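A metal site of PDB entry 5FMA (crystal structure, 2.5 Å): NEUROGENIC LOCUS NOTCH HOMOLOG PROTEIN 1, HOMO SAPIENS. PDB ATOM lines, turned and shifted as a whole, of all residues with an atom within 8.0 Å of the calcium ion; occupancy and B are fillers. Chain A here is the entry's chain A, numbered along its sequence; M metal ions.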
ATOM      1  N   PRO A  28      11.131 -10.970  26.286  1.00  0.00           N
ATOM      2  CA  PRO A  28      12.126 -11.684  27.104  1.00  0.00           C
ATOM      3  C   PRO A  28      12.183 -13.218  26.962  1.00  0.00           C
ATOM      4  O   PRO A  28      13.252 -13.786  27.189  1.00  0.00           O
ATOM      5  CB  PRO A  28      11.780 -11.263  28.541  1.00  0.00           C
ATOM      6  CG  PRO A  28      11.020  -9.996  28.400  1.00  0.00           C
ATOM      7  CD  PRO A  28      10.267 -10.105  27.119  1.00  0.00           C
ATOM      8  N   SER A  29      11.086 -13.866  26.548  1.00  0.00           N
ATOM      9  CA  SER A  29      11.022 -15.331  26.397  1.00  0.00           C
ATOM     10  C   SER A  29      11.692 -15.892  25.129  1.00  0.00           C
ATOM     11  O   SER A  29      11.846 -17.102  25.025  1.00  0.00           O
ATOM     12  CB  SER A  29       9.570 -15.794  26.455  1.00  0.00           C
ATOM     13  OG  SER A  29       8.775 -15.118  25.495  1.00  0.00           O
ATOM     14  N   PHE A  30      12.056 -15.037  24.157  1.00  0.00           N
ATOM     15  CA  PHE A  30      12.695 -15.473  22.903  1.00  0.00           C
ATOM     16  C   PHE A  30      13.915 -14.600  22.578  1.00  0.00           C
ATOM     17  O   PHE A  30      14.038 -13.488  23.091  1.00  0.00           O
ATOM     18  CB  PHE A  30      11.700 -15.388  21.749  1.00  0.00           C
ATOM     19  CG  PHE A  30      10.582 -16.395  21.846  1.00  0.00           C
ATOM     20  CD1 PHE A  30      10.766 -17.700  21.419  1.00  0.00           C
ATOM     21  CD2 PHE A  30       9.379 -16.056  22.437  1.00  0.00           C
ATOM     22  CE1 PHE A  30       9.754 -18.641  21.562  1.00  0.00           C
ATOM     23  CE2 PHE A  30       8.364 -17.013  22.598  1.00  0.00           C
ATOM     24  CZ  PHE A  30       8.553 -18.285  22.134  1.00  0.00           C
ATOM     25  N   GLN A  37      14.487 -18.476  18.508  1.00  0.00           N
ATOM     26  CA  GLN A  37      15.152 -19.351  19.477  1.00  0.00           C
ATOM     27  C   GLN A  37      14.630 -19.037  20.889  1.00  0.00           C
ATOM     28  O   GLN A  37      14.494 -17.868  21.256  1.00  0.00           O
ATOM     29  CB  GLN A  37      16.676 -19.154  19.459  1.00  0.00           C
ATOM     30  CG  GLN A  37      17.341 -19.532  18.140  1.00  0.00           C
ATOM     31  CD  GLN A  37      18.788 -19.122  18.128  1.00  0.00           C
ATOM     32  OE1 GLN A  37      19.161 -18.041  17.623  1.00  0.00           O
ATOM     33  NE2 GLN A  37      19.651 -19.960  18.681  1.00  0.00           N
ATOM     34  N   ASP A  38      14.339 -20.094  21.668  1.00  0.00           N
ATOM     35  CA  ASP A  38      13.819 -19.938  23.028  1.00  0.00           C
ATOM     36  C   ASP A  38      14.957 -19.563  23.989  1.00  0.00           C
ATOM     37  O   ASP A  38      16.060 -20.087  23.864  1.00  0.00           O
ATOM     38  CB  ASP A  38      13.157 -21.250  23.488  1.00  0.00           C
ATOM     39  CG  ASP A  38      12.612 -21.190  24.908  1.00  0.00           C
ATOM     40  OD1 ASP A  38      11.575 -20.533  25.116  1.00  0.00           O
ATOM     41  OD2 ASP A  38      13.266 -21.722  25.807  1.00  0.00           O
ATOM     42  N   VAL A  39      14.660 -18.684  24.979  1.00  0.00           N
ATOM     43  CA  VAL A  39      15.624 -18.373  26.022  1.00  0.00           C
ATOM     44  C   VAL A  39      15.379 -19.400  27.107  1.00  0.00           C
ATOM     45  O   VAL A  39      14.235 -19.672  27.473  1.00  0.00           O
ATOM     46  CB  VAL A  39      15.589 -16.928  26.609  1.00  0.00           C
ATOM     47  CG1 VAL A  39      15.509 -15.879  25.523  1.00  0.00           C
ATOM     48  CG2 VAL A  39      14.499 -16.728  27.661  1.00  0.00           C
ATOM     49  N   ASN A  40      16.464 -19.976  27.626  1.00  0.00           N
ATOM     50  CA  ASN A  40      16.369 -20.925  28.718  1.00  0.00           C
ATOM     51  C   ASN A  40      16.376 -20.111  30.006  1.00  0.00           C
ATOM     52  O   ASN A  40      17.438 -19.632  30.420  1.00  0.00           O
ATOM     53  CB  ASN A  40      17.517 -21.940  28.650  1.00  0.00           C
ATOM     54  CG  ASN A  40      17.491 -22.992  29.741  1.00  0.00           C
ATOM     55  OD1 ASN A  40      16.591 -23.048  30.578  1.00  0.00           O
ATOM     56  ND2 ASN A  40      18.524 -23.819  29.792  1.00  0.00           N
ATOM     57  N   GLU A  41      15.204 -19.920  30.617  1.00  0.00           N
ATOM     58  CA  GLU A  41      15.072 -19.135  31.856  1.00  0.00           C
ATOM     59  C   GLU A  41      15.792 -19.785  33.033  1.00  0.00           C
ATOM     60  O   GLU A  41      16.303 -19.072  33.909  1.00  0.00           O
ATOM     61  CB  GLU A  41      13.586 -18.915  32.217  1.00  0.00           C
ATOM     62  CG  GLU A  41      12.856 -17.910  31.340  1.00  0.00           C
ATOM     63  CD  GLU A  41      12.269 -18.412  30.026  1.00  0.00           C
ATOM     64  OE1 GLU A  41      12.318 -19.634  29.761  1.00  0.00           O
ATOM     65  OE2 GLU A  41      11.746 -17.566  29.259  1.00  0.00           O
ATOM     66  N   CYS A  42      15.842 -21.126  33.084  1.00  0.00           N
ATOM     67  CA  CYS A  42      16.536 -21.871  34.138  1.00  0.00           C
ATOM     68  C   CYS A  42      18.036 -21.584  34.117  1.00  0.00           C
ATOM     69  O   CYS A  42      18.661 -21.437  35.173  1.00  0.00           O
ATOM     70  CB  CYS A  42      16.263 -23.373  33.989  1.00  0.00           C
ATOM     71  SG  CYS A  42      14.535 -23.778  33.657  1.00  0.00           S
ATOM     72  N   GLU A  44      19.552 -18.805  32.738  1.00  0.00           N
ATOM     73  CA  GLU A  44      19.870 -17.390  32.975  1.00  0.00           C
ATOM     74  C   GLU A  44      19.771 -17.032  34.453  1.00  0.00           C
ATOM     75  O   GLU A  44      20.495 -16.133  34.896  1.00  0.00           O
ATOM     76  CB  GLU A  44      19.045 -16.442  32.063  1.00  0.00           C
ATOM     77  CG  GLU A  44      17.652 -16.069  32.538  1.00  0.00           C
ATOM     78  CD  GLU A  44      16.785 -15.359  31.508  1.00  0.00           C
ATOM     79  OE1 GLU A  44      17.341 -14.770  30.543  1.00  0.00           O
ATOM     80  OE2 GLU A  44      15.540 -15.355  31.673  1.00  0.00           O
ATOM     81  N   HIS A  56      12.217 -26.629  34.590  1.00  0.00           N
ATOM     82  CA  HIS A  56      12.025 -27.304  33.310  1.00  0.00           C
ATOM     83  C   HIS A  56      11.752 -26.243  32.254  1.00  0.00           C
ATOM     84  O   HIS A  56      10.763 -25.531  32.348  1.00  0.00           O
ATOM     85  CB  HIS A  56      10.848 -28.277  33.386  1.00  0.00           C
ATOM     86  CG  HIS A  56      11.213 -29.611  33.945  1.00  0.00           C
ATOM     87  ND1 HIS A  56      11.377 -29.801  35.308  1.00  0.00           N
ATOM     88  CD2 HIS A  56      11.457 -30.779  33.313  1.00  0.00           C
ATOM     89  CE1 HIS A  56      11.704 -31.071  35.464  1.00  0.00           C
ATOM     90  NE2 HIS A  56      11.750 -31.704  34.278  1.00  0.00           N
ATOM     91  N   ASN A  57      12.649 -26.118  31.270  1.00  0.00           N
ATOM     92  CA  ASN A  57      12.512 -25.124  30.216  1.00  0.00           C
ATOM     93  C   ASN A  57      11.526 -25.578  29.164  1.00  0.00           C
ATOM     94  O   ASN A  57      11.458 -26.769  28.851  1.00  0.00           O
ATOM     95  CB  ASN A  57      13.864 -24.848  29.567  1.00  0.00           C
ATOM     96  CG  ASN A  57      13.859 -23.693  28.602  1.00  0.00           C
ATOM     97  OD1 ASN A  57      13.179 -22.680  28.805  1.00  0.00           O
ATOM     98  ND2 ASN A  57      14.629 -23.790  27.524  1.00  0.00           N
ATOM     99  N   GLU A  58      10.776 -24.625  28.601  1.00  0.00           N
ATOM    100  CA  GLU A  58       9.764 -24.863  27.568  1.00  0.00           C
ATOM    101  C   GLU A  58       9.876 -23.810  26.467  1.00  0.00           C
ATOM    102  O   GLU A  58      10.536 -22.785  26.662  1.00  0.00           O
ATOM    103  CB  GLU A  58       8.367 -24.779  28.187  1.00  0.00           C
ATOM    104  CG  GLU A  58       8.109 -25.766  29.307  1.00  0.00           C
ATOM    105  CD  GLU A  58       6.695 -25.678  29.839  1.00  0.00           C
ATOM    106  OE1 GLU A  58       6.250 -24.561  30.187  1.00  0.00           O
ATOM    107  OE2 GLU A  58       5.997 -26.727  29.837  1.00  0.00           O
ATOM    108  N   VAL A  59       9.207 -24.037  25.344  1.00  0.00           N
ATOM    109  CA  VAL A  59       9.186 -23.085  24.229  1.00  0.00           C
ATOM    110  C   VAL A  59       8.265 -21.913  24.632  1.00  0.00           C
ATOM    111  O   VAL A  59       7.045 -22.090  24.704  1.00  0.00           O
ATOM    112  CB  VAL A  59       8.701 -23.752  22.918  1.00  0.00           C
ATOM    113  CG1 VAL A  59       8.552 -22.716  21.796  1.00  0.00           C
ATOM    114  CG2 VAL A  59       9.630 -24.883  22.477  1.00  0.00           C
ATOM    115  N   GLY A  60       8.859 -20.754  24.928  1.00  0.00           N
ATOM    116  CA  GLY A  60       8.131 -19.544  25.311  1.00  0.00           C
ATOM    117  C   GLY A  60       7.972 -19.315  26.798  1.00  0.00           C
ATOM    118  O   GLY A  60       7.492 -18.253  27.207  1.00  0.00           O
ATOM    119  N   SER A  61       8.341 -20.304  27.644  1.00  0.00           N
ATOM    120  CA  SER A  61       8.211 -20.171  29.093  1.00  0.00           C
ATOM    121  C   SER A  61       9.075 -21.240  29.798  1.00  0.00           C
ATOM    122  O   SER A  61      10.000 -21.791  29.202  1.00  0.00           O
ATOM    123  CB  SER A  61       6.732 -20.316  29.486  1.00  0.00           C
ATOM    124  OG  SER A  61       6.293 -21.660  29.319  1.00  0.00           O
ATOM    125  N   TYR A  62       8.814 -21.467  31.079  1.00  0.00           N
ATOM    126  CA  TYR A  62       9.465 -22.491  31.885  1.00  0.00           C
ATOM    127  C   TYR A  62       8.461 -22.952  32.924  1.00  0.00           C
ATOM    128  O   TYR A  62       7.493 -22.216  33.195  1.00  0.00           O
ATOM    129  CB  TYR A  62      10.735 -21.936  32.562  1.00  0.00           C
ATOM    130  CG  TYR A  62      10.454 -20.894  33.617  1.00  0.00           C
ATOM    131  CD1 TYR A  62      10.205 -19.570  33.278  1.00  0.00           C
ATOM    132  CD2 TYR A  62      10.374 -21.247  34.963  1.00  0.00           C
ATOM    133  CE1 TYR A  62       9.901 -18.614  34.241  1.00  0.00           C
ATOM    134  CE2 TYR A  62      10.071 -20.299  35.941  1.00  0.00           C
ATOM    135  CZ  TYR A  62       9.829 -18.988  35.575  1.00  0.00           C
ATOM    136  OH  TYR A  62       9.550 -18.030  36.510  1.00  0.00           O
ATOM    137  N   ARG A  63       8.660 -24.123  33.520  1.00  0.00           N
ATOM    138  CA  ARG A  63       7.773 -24.612  34.583  1.00  0.00           C
ATOM    139  C   ARG A  63       8.621 -25.124  35.733  1.00  0.00           C
ATOM    140  O   ARG A  63       9.708 -25.661  35.507  1.00  0.00           O
ATOM    141  CB  ARG A  63       6.791 -25.685  34.067  1.00  0.00           C
ATOM    142  CG  ARG A  63       7.416 -27.017  33.688  1.00  0.00           C
ATOM    143  CD  ARG A  63       6.368 -27.970  33.155  1.00  0.00           C
ATOM    144  NE  ARG A  63       6.854 -29.351  33.100  1.00  0.00           N
ATOM    145  CZ  ARG A  63       7.635 -29.854  32.144  1.00  0.00           C
ATOM    146  NH1 ARG A  63       8.044 -29.094  31.127  1.00  0.00           N
ATOM    147  NH2 ARG A  63       8.020 -31.129  32.193  1.00  0.00           N
HETATM  148 CA    CA M   1      11.966 -20.943  27.805  1.00  0.00          CA
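The backbone NH (N) of Gly 60 sits close to the side-chain carboxylate (OD1) of Asp 38 (2.7 Å). The side-chain hydroxyl (OG) of Ser 61 lies within hydrogen-bond range of the side-chain carboxylate (OE1) of Glu 58 (3.0 Å). The guanidinium group (NH1) of Arg 63 is in salt-bridge range of the side-chain carboxylate (OE2) of Glu 58. The backbone carbonyl oxygen (O) of Ser 29 sits at hydrogen-bond distance from the backbone NH (N) of Val 39.
Within 4 Å of the calcium ion: Asp 38, Val 39, Glu 41, Asn 57, Glu 58 and Ser 61.
The calcium ion is bound by OD1 of Asn 57 (2.3 Å), OE1 of Glu 41 (2.4 Å), OD2 of Asp 38 (2.5 Å), O of Ser 61 (2.6 Å), O of Glu 58 (2.6 Å), O of Val 39 (2.6 Å) and OD1 of Asp 38 (2.7 Å).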
